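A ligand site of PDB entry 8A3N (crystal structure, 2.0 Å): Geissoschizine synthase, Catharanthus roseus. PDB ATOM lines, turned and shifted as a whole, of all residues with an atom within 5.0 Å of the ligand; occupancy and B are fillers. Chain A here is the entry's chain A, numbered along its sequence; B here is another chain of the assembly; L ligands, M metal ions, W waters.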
ATOM      1  N   CYS A  52       2.759  24.338  17.474  1.00  0.00           N
ATOM      2  CA  CYS A  52       3.178  24.969  16.239  1.00  0.00           C
ATOM      3  C   CYS A  52       3.611  26.413  16.493  1.00  0.00           C
ATOM      4  O   CYS A  52       3.619  26.868  17.631  1.00  0.00           O
ATOM      5  CB  CYS A  52       2.070  24.924  15.201  1.00  0.00           C
ATOM      6  SG  CYS A  52       0.732  26.098  15.520  1.00  0.00           S
ATOM      7  N   ASN A  53       4.024  27.082  15.415  1.00  0.00           N
ATOM      8  CA  ASN A  53       4.481  28.461  15.425  1.00  0.00           C
ATOM      9  C   ASN A  53       3.510  29.370  16.161  1.00  0.00           C
ATOM     10  O   ASN A  53       3.941  30.224  16.936  1.00  0.00           O
ATOM     11  CB  ASN A  53       4.744  28.915  13.977  1.00  0.00           C
ATOM     12  CG  ASN A  53       4.937  30.403  13.843  1.00  0.00           C
ATOM     13  OD1 ASN A  53       3.965  31.152  13.671  1.00  0.00           O
ATOM     14  ND2 ASN A  53       6.178  30.840  13.880  1.00  0.00           N
ATOM     15  N   PHE A  54       2.202  29.188  15.914  1.00  0.00           N
ATOM     16  CA  PHE A  54       1.185  30.020  16.533  1.00  0.00           C
ATOM     17  C   PHE A  54       1.288  29.954  18.053  1.00  0.00           C
ATOM     18  O   PHE A  54       1.279  30.988  18.710  1.00  0.00           O
ATOM     19  CB  PHE A  54      -0.209  29.601  16.063  1.00  0.00           C
ATOM     20  CG  PHE A  54      -1.334  30.391  16.676  1.00  0.00           C
ATOM     21  CD1 PHE A  54      -1.655  31.650  16.198  1.00  0.00           C
ATOM     22  CD2 PHE A  54      -2.064  29.891  17.751  1.00  0.00           C
ATOM     23  CE1 PHE A  54      -2.692  32.382  16.763  1.00  0.00           C
ATOM     24  CE2 PHE A  54      -3.100  30.624  18.316  1.00  0.00           C
ATOM     25  CZ  PHE A  54      -3.404  31.879  17.824  1.00  0.00           C
ATOM     26  N   TRP A  63       1.332  38.941  19.436  1.00  0.00           N
ATOM     27  CA  TRP A  63       0.320  39.662  18.679  1.00  0.00           C
ATOM     28  C   TRP A  63      -0.699  40.351  19.587  1.00  0.00           C
ATOM     29  O   TRP A  63      -1.638  40.966  19.078  1.00  0.00           O
ATOM     30  CB  TRP A  63      -0.385  38.716  17.709  1.00  0.00           C
ATOM     31  CG  TRP A  63       0.525  38.091  16.704  1.00  0.00           C
ATOM     32  CD1 TRP A  63       1.313  38.736  15.792  1.00  0.00           C
ATOM     33  CD2 TRP A  63       0.749  36.690  16.507  1.00  0.00           C
ATOM     34  NE1 TRP A  63       2.015  37.837  15.043  1.00  0.00           N
ATOM     35  CE2 TRP A  63       1.677  36.563  15.446  1.00  0.00           C
ATOM     36  CE3 TRP A  63       0.232  35.523  17.084  1.00  0.00           C
ATOM     37  CZ2 TRP A  63       2.117  35.329  14.975  1.00  0.00           C
ATOM     38  CZ3 TRP A  63       0.669  34.301  16.620  1.00  0.00           C
ATOM     39  CH2 TRP A  63       1.587  34.209  15.581  1.00  0.00           C
ATOM     40  N   CYS A 169      -4.397  21.654  12.148  1.00  0.00           N
ATOM     41  CA  CYS A 169      -3.895  23.000  11.939  1.00  0.00           C
ATOM     42  C   CYS A 169      -3.366  23.117  10.508  1.00  0.00           C
ATOM     43  O   CYS A 169      -3.922  23.873   9.718  1.00  0.00           O
ATOM     44  CB  CYS A 169      -2.821  23.252  12.983  1.00  0.00           C
ATOM     45  SG  CYS A 169      -1.962  24.843  12.840  1.00  0.00           S
ATOM     46  N   VAL A 173      -6.205  24.616   7.419  1.00  0.00           N
ATOM     47  CA  VAL A 173      -5.896  25.973   7.008  1.00  0.00           C
ATOM     48  C   VAL A 173      -5.742  26.046   5.481  1.00  0.00           C
ATOM     49  O   VAL A 173      -6.118  27.043   4.878  1.00  0.00           O
ATOM     50  CB  VAL A 173      -4.646  26.519   7.721  1.00  0.00           C
ATOM     51  CG1 VAL A 173      -4.202  27.865   7.137  1.00  0.00           C
ATOM     52  CG2 VAL A 173      -4.835  26.641   9.234  1.00  0.00           C
ATOM     53  N   GLY A 194       6.781  28.145   0.868  1.00  0.00           N
ATOM     54  CA  GLY A 194       7.179  27.733   2.195  1.00  0.00           C
ATOM     55  C   GLY A 194       6.812  26.280   2.444  1.00  0.00           C
ATOM     56  O   GLY A 194       5.632  25.945   2.491  1.00  0.00           O
ATOM     57  N   LEU A 195       7.827  25.427   2.569  1.00  0.00           N
ATOM     58  CA  LEU A 195       7.591  24.025   2.822  1.00  0.00           C
ATOM     59  C   LEU A 195       7.831  23.706   4.303  1.00  0.00           C
ATOM     60  O   LEU A 195       8.862  23.148   4.662  1.00  0.00           O
ATOM     61  CB  LEU A 195       8.487  23.183   1.914  1.00  0.00           C
ATOM     62  CG  LEU A 195       8.165  21.700   1.898  1.00  0.00           C
ATOM     63  CD1 LEU A 195       6.851  21.442   1.161  1.00  0.00           C
ATOM     64  CD2 LEU A 195       9.312  20.915   1.261  1.00  0.00           C
ATOM     65  N   GLY A 196       6.857  24.081   5.131  1.00  0.00           N
ATOM     66  CA  GLY A 196       6.774  23.597   6.500  1.00  0.00           C
ATOM     67  C   GLY A 196       5.550  22.714   6.658  1.00  0.00           C
ATOM     68  O   GLY A 196       5.162  22.022   5.721  1.00  0.00           O
ATOM     69  N   GLY A 197       4.928  22.765   7.841  1.00  0.00           N
ATOM     70  CA  GLY A 197       3.727  22.003   8.118  1.00  0.00           C
ATOM     71  C   GLY A 197       2.609  22.280   7.107  1.00  0.00           C
ATOM     72  O   GLY A 197       2.086  21.360   6.484  1.00  0.00           O
ATOM     73  N   LEU A 198       2.213  23.557   6.983  1.00  0.00           N
ATOM     74  CA  LEU A 198       1.128  23.920   6.070  1.00  0.00           C
ATOM     75  C   LEU A 198       1.525  23.589   4.630  1.00  0.00           C
ATOM     76  O   LEU A 198       0.752  22.959   3.908  1.00  0.00           O
ATOM     77  CB  LEU A 198       0.807  25.408   6.192  1.00  0.00           C
ATOM     78  CG  LEU A 198      -0.318  25.760   7.158  1.00  0.00           C
ATOM     79  CD1 LEU A 198       0.116  25.559   8.602  1.00  0.00           C
ATOM     80  CD2 LEU A 198      -0.784  27.187   6.925  1.00  0.00           C
ATOM     81  N   GLY A 199       2.729  24.026   4.246  1.00  0.00           N
ATOM     82  CA  GLY A 199       3.217  23.835   2.897  1.00  0.00           C
ATOM     83  C   GLY A 199       3.205  22.374   2.469  1.00  0.00           C
ATOM     84  O   GLY A 199       2.681  22.048   1.402  1.00  0.00           O
ATOM     85  N   ILE A 216       7.948  26.677  -3.840  1.00  0.00           N
ATOM     86  CA  ILE A 216       8.974  27.697  -3.782  1.00  0.00           C
ATOM     87  C   ILE A 216       9.427  27.834  -2.325  1.00  0.00           C
ATOM     88  O   ILE A 216       8.629  28.209  -1.471  1.00  0.00           O
ATOM     89  CB  ILE A 216       8.488  29.046  -4.355  1.00  0.00           C
ATOM     90  CG1 ILE A 216       7.916  28.918  -5.767  1.00  0.00           C
ATOM     91  CG2 ILE A 216       9.592  30.079  -4.297  1.00  0.00           C
ATOM     92  CD1 ILE A 216       6.455  28.496  -5.830  1.00  0.00           C
ATOM     93  N   SER A 217      10.707  27.561  -2.071  1.00  0.00           N
ATOM     94  CA  SER A 217      11.268  27.453  -0.734  1.00  0.00           C
ATOM     95  C   SER A 217      12.524  28.318  -0.627  1.00  0.00           C
ATOM     96  O   SER A 217      13.156  28.614  -1.635  1.00  0.00           O
ATOM     97  CB  SER A 217      11.572  26.000  -0.436  1.00  0.00           C
ATOM     98  OG  SER A 217      12.376  25.840   0.731  1.00  0.00           O
ATOM     99  N   THR A 218      12.883  28.709   0.608  1.00  0.00           N
ATOM    100  CA  THR A 218      14.140  29.400   0.878  1.00  0.00           C
ATOM    101  C   THR A 218      15.265  28.395   1.120  1.00  0.00           C
ATOM    102  O   THR A 218      16.434  28.787   1.099  1.00  0.00           O
ATOM    103  CB  THR A 218      14.030  30.364   2.064  1.00  0.00           C
ATOM    104  OG1 THR A 218      13.767  29.632   3.269  1.00  0.00           O
ATOM    105  CG2 THR A 218      12.960  31.423   1.869  1.00  0.00           C
ATOM    106  N   SER A 219      14.911  27.125   1.368  1.00  0.00           N
ATOM    107  CA  SER A 219      15.859  26.065   1.732  1.00  0.00           C
ATOM    108  C   SER A 219      16.097  25.122   0.554  1.00  0.00           C
ATOM    109  O   SER A 219      15.247  24.268   0.260  1.00  0.00           O
ATOM    110  CB  SER A 219      15.359  25.260   2.923  1.00  0.00           C
ATOM    111  OG  SER A 219      14.861  26.092   3.971  1.00  0.00           O
ATOM    112  N   LYS A 222      15.697  21.241   1.004  1.00  0.00           N
ATOM    113  CA  LYS A 222      14.375  20.625   1.069  1.00  0.00           C
ATOM    114  C   LYS A 222      13.922  20.077  -0.299  1.00  0.00           C
ATOM    115  O   LYS A 222      12.833  19.512  -0.406  1.00  0.00           O
ATOM    116  CB  LYS A 222      13.354  21.636   1.603  1.00  0.00           C
ATOM    117  CG  LYS A 222      13.504  21.986   3.076  1.00  0.00           C
ATOM    118  CD  LYS A 222      12.395  22.872   3.608  1.00  0.00           C
ATOM    119  CE  LYS A 222      12.463  23.051   5.114  1.00  0.00           C
ATOM    120  NZ  LYS A 222      11.386  23.956   5.600  1.00  0.00           N
ATOM    121  N   THR A 257       2.265  30.347   2.578  1.00  0.00           N
ATOM    122  CA  THR A 257       2.363  29.966   3.984  1.00  0.00           C
ATOM    123  C   THR A 257       3.464  30.747   4.690  1.00  0.00           C
ATOM    124  O   THR A 257       3.636  30.588   5.892  1.00  0.00           O
ATOM    125  CB  THR A 257       2.587  28.459   4.169  1.00  0.00           C
ATOM    126  OG1 THR A 257       3.980  28.153   4.056  1.00  0.00           O
ATOM    127  CG2 THR A 257       1.780  27.626   3.206  1.00  0.00           C
ATOM    128  N   THR A 258       4.200  31.604   3.966  1.00  0.00           N
ATOM    129  CA  THR A 258       5.251  32.412   4.564  1.00  0.00           C
ATOM    130  C   THR A 258       4.639  33.539   5.384  1.00  0.00           C
ATOM    131  O   THR A 258       3.482  33.906   5.154  1.00  0.00           O
ATOM    132  CB  THR A 258       6.212  32.976   3.514  1.00  0.00           C
ATOM    133  OG1 THR A 258       5.529  33.985   2.767  1.00  0.00           O
ATOM    134  CG2 THR A 258       6.751  31.915   2.568  1.00  0.00           C
ATOM    135  N   PRO A 259       5.380  34.152   6.342  1.00  0.00           N
ATOM    136  CA  PRO A 259       4.863  35.297   7.078  1.00  0.00           C
ATOM    137  C   PRO A 259       4.473  36.392   6.099  1.00  0.00           C
ATOM    138  O   PRO A 259       5.183  36.648   5.136  1.00  0.00           O
ATOM    139  CB  PRO A 259       6.006  35.699   8.020  1.00  0.00           C
ATOM    140  CG  PRO A 259       6.881  34.455   8.109  1.00  0.00           C
ATOM    141  CD  PRO A 259       6.750  33.789   6.758  1.00  0.00           C
ATOM    142  N   ARG A 262       6.664  38.597   3.529  1.00  0.00           N
ATOM    143  CA  ARG A 262       7.969  38.011   3.291  1.00  0.00           C
ATOM    144  C   ARG A 262       8.109  37.577   1.835  1.00  0.00           C
ATOM    145  O   ARG A 262       9.218  37.519   1.313  1.00  0.00           O
ATOM    146  CB  ARG A 262       8.223  36.858   4.276  1.00  0.00           C
ATOM    147  CG  ARG A 262       8.401  37.321   5.715  1.00  0.00           C
ATOM    148  CD  ARG A 262       9.648  38.167   5.935  1.00  0.00           C
ATOM    149  NE  ARG A 262      10.841  37.417   5.581  1.00  0.00           N
ATOM    150  CZ  ARG A 262      12.081  37.762   5.906  1.00  0.00           C
ATOM    151  NH1 ARG A 262      12.310  38.815   6.668  1.00  0.00           N
ATOM    152  NH2 ARG A 262      13.093  37.024   5.466  1.00  0.00           N
ATOM    153  N   VAL A 281      -2.354  32.702   3.892  1.00  0.00           N
ATOM    154  CA  VAL A 281      -2.685  32.047   5.151  1.00  0.00           C
ATOM    155  C   VAL A 281      -1.618  32.314   6.210  1.00  0.00           C
ATOM    156  O   VAL A 281      -1.861  32.002   7.378  1.00  0.00           O
ATOM    157  CB  VAL A 281      -2.920  30.543   4.944  1.00  0.00           C
ATOM    158  CG1 VAL A 281      -4.150  30.294   4.075  1.00  0.00           C
ATOM    159  CG2 VAL A 281      -1.707  29.816   4.381  1.00  0.00           C
ATOM    160  N   GLY A 282      -0.468  32.892   5.850  1.00  0.00           N
ATOM    161  CA  GLY A 282       0.607  33.096   6.793  1.00  0.00           C
ATOM    162  C   GLY A 282       0.317  34.207   7.797  1.00  0.00           C
ATOM    163  O   GLY A 282      -0.520  35.073   7.549  1.00  0.00           O
ATOM    164  N   ALA A 283       0.999  34.177   8.947  1.00  0.00           N
ATOM    165  CA  ALA A 283       0.855  35.207   9.969  1.00  0.00           C
ATOM    166  C   ALA A 283       1.281  36.556   9.399  1.00  0.00           C
ATOM    167  O   ALA A 283       2.415  36.702   8.946  1.00  0.00           O
ATOM    168  CB  ALA A 283       1.690  34.879  11.186  1.00  0.00           C
ATOM    169  N   SER A 305      -7.545  33.620   4.517  1.00  0.00           N
ATOM    170  CA  SER A 305      -8.331  32.551   5.107  1.00  0.00           C
ATOM    171  C   SER A 305      -7.779  32.185   6.483  1.00  0.00           C
ATOM    172  O   SER A 305      -6.564  32.160   6.665  1.00  0.00           O
ATOM    173  CB  SER A 305      -8.375  31.361   4.180  1.00  0.00           C
ATOM    174  OG  SER A 305      -9.376  30.442   4.593  1.00  0.00           O
ATOM    175  N   SER A 306      -8.680  31.912   7.431  1.00  0.00           N
ATOM    176  CA  SER A 306      -8.274  31.436   8.741  1.00  0.00           C
ATOM    177  C   SER A 306      -9.043  30.171   9.101  1.00  0.00           C
ATOM    178  O   SER A 306     -10.251  30.084   8.925  1.00  0.00           O
ATOM    179  CB  SER A 306      -8.441  32.509   9.766  1.00  0.00           C
ATOM    180  OG  SER A 306      -9.715  33.096   9.625  1.00  0.00           O
ATOM    181  N   THR A 307      -8.272  29.165   9.562  1.00  0.00           N
ATOM    182  CA  THR A 307      -8.722  27.823   9.873  1.00  0.00           C
ATOM    183  C   THR A 307      -9.845  27.389   8.935  1.00  0.00           C
ATOM    184  O   THR A 307      -9.698  27.464   7.708  1.00  0.00           O
ATOM    185  CB  THR A 307      -9.030  27.688  11.376  1.00  0.00           C
ATOM    186  OG1 THR A 307     -10.189  28.477  11.681  1.00  0.00           O
ATOM    187  CG2 THR A 307      -7.879  28.139  12.255  1.00  0.00           C
ATOM    188  N   ILE A 344      11.127  25.163  17.176  1.00  0.00           N
ATOM    189  CA  ILE A 344      10.069  25.702  16.349  1.00  0.00           C
ATOM    190  C   ILE A 344      10.493  27.067  15.808  1.00  0.00           C
ATOM    191  O   ILE A 344      10.337  27.340  14.623  1.00  0.00           O
ATOM    192  CB  ILE A 344       8.726  25.784  17.116  1.00  0.00           C
ATOM    193  CG1 ILE A 344       8.185  24.385  17.408  1.00  0.00           C
ATOM    194  CG2 ILE A 344       7.702  26.618  16.363  1.00  0.00           C
ATOM    195  CD1 ILE A 344       6.992  24.358  18.324  1.00  0.00           C
ATOM    196  N   LEU A 347      13.153  26.909  13.138  1.00  0.00           N
ATOM    197  CA  LEU A 347      12.760  26.126  11.973  1.00  0.00           C
ATOM    198  C   LEU A 347      13.576  24.827  11.901  1.00  0.00           C
ATOM    199  O   LEU A 347      14.015  24.424  10.822  1.00  0.00           O
ATOM    200  CB  LEU A 347      12.929  26.978  10.710  1.00  0.00           C
ATOM    201  CG  LEU A 347      12.230  28.340  10.742  1.00  0.00           C
ATOM    202  CD1 LEU A 347      12.532  29.119   9.477  1.00  0.00           C
ATOM    203  CD2 LEU A 347      10.723  28.170  10.929  1.00  0.00           C
ATOM    204  N   TYR A 351       7.918  18.395  10.391  1.00  0.00           N
ATOM    205  CA  TYR A 351       7.814  19.849  10.374  1.00  0.00           C
ATOM    206  C   TYR A 351       7.106  20.349  11.634  1.00  0.00           C
ATOM    207  O   TYR A 351       7.067  21.558  11.880  1.00  0.00           O
ATOM    208  CB  TYR A 351       7.008  20.338   9.168  1.00  0.00           C
ATOM    209  CG  TYR A 351       7.611  19.920   7.854  1.00  0.00           C
ATOM    210  CD1 TYR A 351       8.758  20.540   7.381  1.00  0.00           C
ATOM    211  CD2 TYR A 351       7.060  18.880   7.121  1.00  0.00           C
ATOM    212  CE1 TYR A 351       9.338  20.144   6.186  1.00  0.00           C
ATOM    213  CE2 TYR A 351       7.640  18.475   5.927  1.00  0.00           C
ATOM    214  CZ  TYR A 351       8.776  19.116   5.456  1.00  0.00           C
ATOM    215  OH  TYR A 351       9.353  18.726   4.292  1.00  0.00           O
ATOM    216  N   ARG A 352       6.543  19.414  12.409  1.00  0.00           N
ATOM    217  CA  ARG A 352       5.725  19.723  13.570  1.00  0.00           C
ATOM    218  C   ARG A 352       6.096  18.781  14.709  1.00  0.00           C
ATOM    219  O   ARG A 352       6.516  17.652  14.474  1.00  0.00           O
ATOM    220  CB  ARG A 352       4.241  19.554  13.251  1.00  0.00           C
ATOM    221  CG  ARG A 352       3.672  20.598  12.302  1.00  0.00           C
ATOM    222  CD  ARG A 352       3.677  21.986  12.888  1.00  0.00           C
ATOM    223  NE  ARG A 352       2.933  22.904  12.055  1.00  0.00           N
ATOM    224  CZ  ARG A 352       1.644  23.163  12.181  1.00  0.00           C
ATOM    225  NH1 ARG A 352       0.898  22.422  12.976  1.00  0.00           N
ATOM    226  NH2 ARG A 352       1.089  24.149  11.487  1.00  0.00           N
ATOM    227  N   ILE B 296      -7.461  37.851   6.001  1.00  0.00           N
ATOM    228  CA  ILE B 296      -7.440  36.558   6.651  1.00  0.00           C
ATOM    229  C   ILE B 296      -8.586  36.430   7.656  1.00  0.00           C
ATOM    230  O   ILE B 296      -9.281  35.423   7.668  1.00  0.00           O
ATOM    231  CB  ILE B 296      -6.061  36.328   7.312  1.00  0.00           C
ATOM    232  CG1 ILE B 296      -4.977  36.135   6.247  1.00  0.00           C
ATOM    233  CG2 ILE B 296      -6.093  35.184   8.320  1.00  0.00           C
ATOM    234  CD1 ILE B 296      -3.571  35.986   6.802  1.00  0.00           C
HETATM  235  P1  LIG L   1       6.664  27.380  10.191  1.00  0.00           P
HETATM  236  O1  LIG L   1       7.091  28.307  11.262  1.00  0.00           O
HETATM  237  O2  LIG L   1       7.005  25.935  10.314  1.00  0.00           O
HETATM  238  O3  LIG L   1       7.189  27.933   8.797  1.00  0.00           O
HETATM  239  C1  LIG L   1       6.794  27.228   7.613  1.00  0.00           C
HETATM  240  C2  LIG L   1       7.774  27.528   6.517  1.00  0.00           C
HETATM  241  O4  LIG L   1       7.657  28.931   6.147  1.00  0.00           O
HETATM  242  C3  LIG L   1       9.265  27.386   6.863  1.00  0.00           C
HETATM  243  O5  LIG L   1       9.690  26.033   6.803  1.00  0.00           O
HETATM  244  C4  LIG L   1       9.862  28.212   5.723  1.00  0.00           C
HETATM  245  O6  LIG L   1       9.747  27.433   4.550  1.00  0.00           O
HETATM  246  C5  LIG L   1       8.891  29.386   5.650  1.00  0.00           C
HETATM  247  N1  LIG L   1       9.301  30.537   6.428  1.00  0.00           N
HETATM  248  C6  LIG L   1       9.319  30.657   7.801  1.00  0.00           C
HETATM  249  N2  LIG L   1       9.756  31.821   8.208  1.00  0.00           N
HETATM  250  C7  LIG L   1      10.047  32.506   7.038  1.00  0.00           C
HETATM  251  C8  LIG L   1      10.522  33.807   6.792  1.00  0.00           C
HETATM  252  N3  LIG L   1      10.827  34.656   7.768  1.00  0.00           N
HETATM  253  N4  LIG L   1      10.687  34.186   5.507  1.00  0.00           N
HETATM  254  C9  LIG L   1      10.402  33.305   4.536  1.00  0.00           C
HETATM  255  N5  LIG L   1       9.925  32.062   4.644  1.00  0.00           N
HETATM  256  C10 LIG L   1       9.768  31.724   5.935  1.00  0.00           C
HETATM  257  O7  LIG L   1       5.082  27.535   9.924  1.00  0.00           O
HETATM  258  P2  LIG L   1       3.809  26.581   9.660  1.00  0.00           P
HETATM  259  O8  LIG L   1       3.981  25.811   8.392  1.00  0.00           O
HETATM  260  O9  LIG L   1       3.467  25.856  10.917  1.00  0.00           O
HETATM  261  O10 LIG L   1       2.678  27.712   9.432  1.00  0.00           O
HETATM  262  C11 LIG L   1       2.790  28.591   8.294  1.00  0.00           C
HETATM  263  C12 LIG L   1       2.210  29.944   8.619  1.00  0.00           C
HETATM  264  O11 LIG L   1       0.780  29.838   8.804  1.00  0.00           O
HETATM  265  C13 LIG L   1       2.739  30.612   9.894  1.00  0.00           C
HETATM  266  O12 LIG L   1       2.939  32.002   9.672  1.00  0.00           O
HETATM  267  C14 LIG L   1       1.645  30.311  10.927  1.00  0.00           C
HETATM  268  O13 LIG L   1       1.615  31.193  12.033  1.00  0.00           O
HETATM  269  C15 LIG L   1       0.426  30.492  10.014  1.00  0.00           C
HETATM  270  N6  LIG L   1      -0.863  29.935  10.485  1.00  0.00           N
HETATM  271  C16 LIG L   1      -2.011  30.403   9.901  1.00  0.00           C
HETATM  272  C17 LIG L   1      -3.254  29.931  10.297  1.00  0.00           C
HETATM  273  C18 LIG L   1      -4.479  30.460   9.619  1.00  0.00           C
HETATM  274  O14 LIG L   1      -5.593  30.075   9.999  1.00  0.00           O
HETATM  275  N7  LIG L   1      -4.342  31.285   8.594  1.00  0.00           N
HETATM  276  C19 LIG L   1      -3.324  28.962  11.295  1.00  0.00           C
HETATM  277  C20 LIG L   1      -2.163  28.492  11.874  1.00  0.00           C
HETATM  278  C21 LIG L   1      -0.938  28.974  11.468  1.00  0.00           C
HETATM  279  P3  LIG L   1      11.093  27.194   3.706  1.00  0.00           P
HETATM  280  O15 LIG L   1      10.616  26.323   2.577  1.00  0.00           O
HETATM  281  O16 LIG L   1      12.104  26.479   4.606  1.00  0.00           O
HETATM  282  O17 LIG L   1      11.580  28.547   3.242  1.00  0.00           O
HETATM  283 ZN    ZN M   1      -1.211  24.900  15.035  1.00  0.00          ZN
HETATM  284  O   HOH W   1       6.487  31.083  10.346  1.00  0.00           O
HETATM  285  O   HOH W   2       8.926  24.491   8.942  1.00  0.00           O
HETATM  286  O   HOH W   3       1.768  27.566  12.815  1.00  0.00           O
HETATM  287  O   HOH W   4       4.525  25.824   5.801  1.00  0.00           O
HETATM  288  O   HOH W   5      12.912  35.373   3.253  1.00  0.00           O
HETATM  289  O   HOH W   6       9.722  30.244   2.569  1.00  0.00           O
HETATM  290  O   HOH W   7      -4.960  26.350  12.941  1.00  0.00           O
HETATM  291  O   HOH W   8       5.726  30.797   7.714  1.00  0.00           O
HETATM  292  O   HOH W   9       8.906  25.464  12.871  1.00  0.00           O
HETATM  293  O   HOH W  10       8.250  29.189  13.946  1.00  0.00           O
HETATM  294  O   HOH W  11       5.624  23.711  10.479  1.00  0.00           O
HETATM  295  O   HOH W  12       4.533  32.926  11.773  1.00  0.00           O
HETATM  296  O   HOH W  13       4.791  25.623  13.202  1.00  0.00           O
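Water W11 lies within hydrogen-bond range of O2 of the ligand, N of Gly 197, O of Tyr 351 and NE of Arg 352. Water W13 lies within hydrogen-bond range of O9 of the ligand, N of Asn 53 and NE of Arg 352. Water W12 lies within hydrogen-bond range of the side-chain amide oxygen (OD1) of Asn 53 (2.7 Å) and an oxygen (O12) of the ligand (2.8 Å). Water W10 lies within hydrogen-bond range of the side-chain amide nitrogen of Asn 53 (2.7 Å), the backbone carbonyl oxygen of Ile 344 (2.9 Å) and an oxygen (O1) of the ligand (3.1 Å). Water W9 lies within hydrogen-bond range of the backbone carbonyl oxygen of Ile 344 (2.9 Å) and an oxygen (O2) of the ligand (3.2 Å). Water W5 lies within hydrogen-bond range of NH2 of Arg 262 (2.8 Å) and N4 of the ligand (3.4 Å).
OG1 of Thr 218 lies within hydrogen-bond range of O17 of the ligand (2.4 Å). NH2 of Arg 352 lies within salt-bridge range of O9 of the ligand (3.0 Å). OG of Ser 219 is in hydrogen-bond range of O16 of the ligand (2.9 Å). O of Ser 305 is in hydrogen-bond range of N7 of the ligand, at 3.1 Å. A nitrogen (N7) of the ligand sits at hydrogen-bond distance from the backbone carbonyl oxygen (O) of Val 281, at 2.9 Å. The backbone NH (N) of Thr 307 sits at hydrogen-bond distance from an oxygen (O14) of the ligand. An oxygen (O17) of the ligand lies within hydrogen-bond range of the backbone NH of Thr 218 (2.9 Å). The backbone NH (N) of Leu 195 is in hydrogen-bond range of an oxygen (O15) of the ligand, 2.9 Å away. O8 of the ligand sits at hydrogen-bond distance from N of Leu 198. An oxygen (O8) of the ligand lies within hydrogen-bond range of the backbone NH (N) of Gly 197. The guanidinium group (NE) of Arg 262 sits at hydrogen-bond distance from a nitrogen (N4) of the ligand, at 3.2 Å. The side-chain amide oxygen of Asn 53 sits at hydrogen-bond distance from an oxygen (O13) of the ligand (2.9 Å). The side-chain amino group (NZ) of Lys 222 is in salt-bridge range of an oxygen (O16) of the ligand. The side-chain hydroxyl of Ser 217 lies within hydrogen-bond range of an oxygen (O15) of the ligand. An oxygen (O12) of the ligand is in hydrogen-bond range of the backbone NH (N) of Ala 283, 3.0 Å away.
The side-chain hydroxyl of Ser 217 is in hydrogen-bond range of the backbone NH of Ser 219. The backbone carbonyl oxygen of Ile 216 sits at hydrogen-bond distance from the backbone NH of Gly 194 (3.0 Å). NH2 of Arg 352 lies close to SG of Cys 169. The side-chain amino group (NZ) of Lys 222 lies within hydrogen-bond range of the backbone carbonyl oxygen (O) of Leu 195 (2.8 Å). The backbone carbonyl oxygen (O) of Gly 194 is in hydrogen-bond range of the side-chain hydroxyl (OG1) of Thr 257 (3.2 Å). The side-chain hydroxyl of Ser 306 is in hydrogen-bond range of the backbone carbonyl oxygen of Ile 296 of chain B (3.1 Å).
Cys 169 touches the ligand. Val 173 touches the ligand (CG2 to C19, 3.5 Å). Gly 194 touches the ligand (CA to O6, 3.5 Å). Gly 196 touches the ligand (CA to C1, 3.8 Å). O of Thr 257 touches C12 of the ligand, 3.1 Å away. CG2 of Thr 258 touches N5 of the ligand (3.8 Å). CD of Pro 259 touches C7 of the ligand, 3.5 Å away. CA of Gly 282 touches O11 of the ligand, at 3.8 Å. Ser 306 touches the ligand (CA to O14, 3.3 Å). Leu 347 touches the ligand (CD2 to O1, 3.6 Å). Hydrophobic or aromatic side chains that line the ligand: Val 173, Leu 195, Leu 198, Pro 259, Val 281, Ala 283 and Leu 347. Of the 32 residues printed, 24 come within 4 Å of the ligand.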
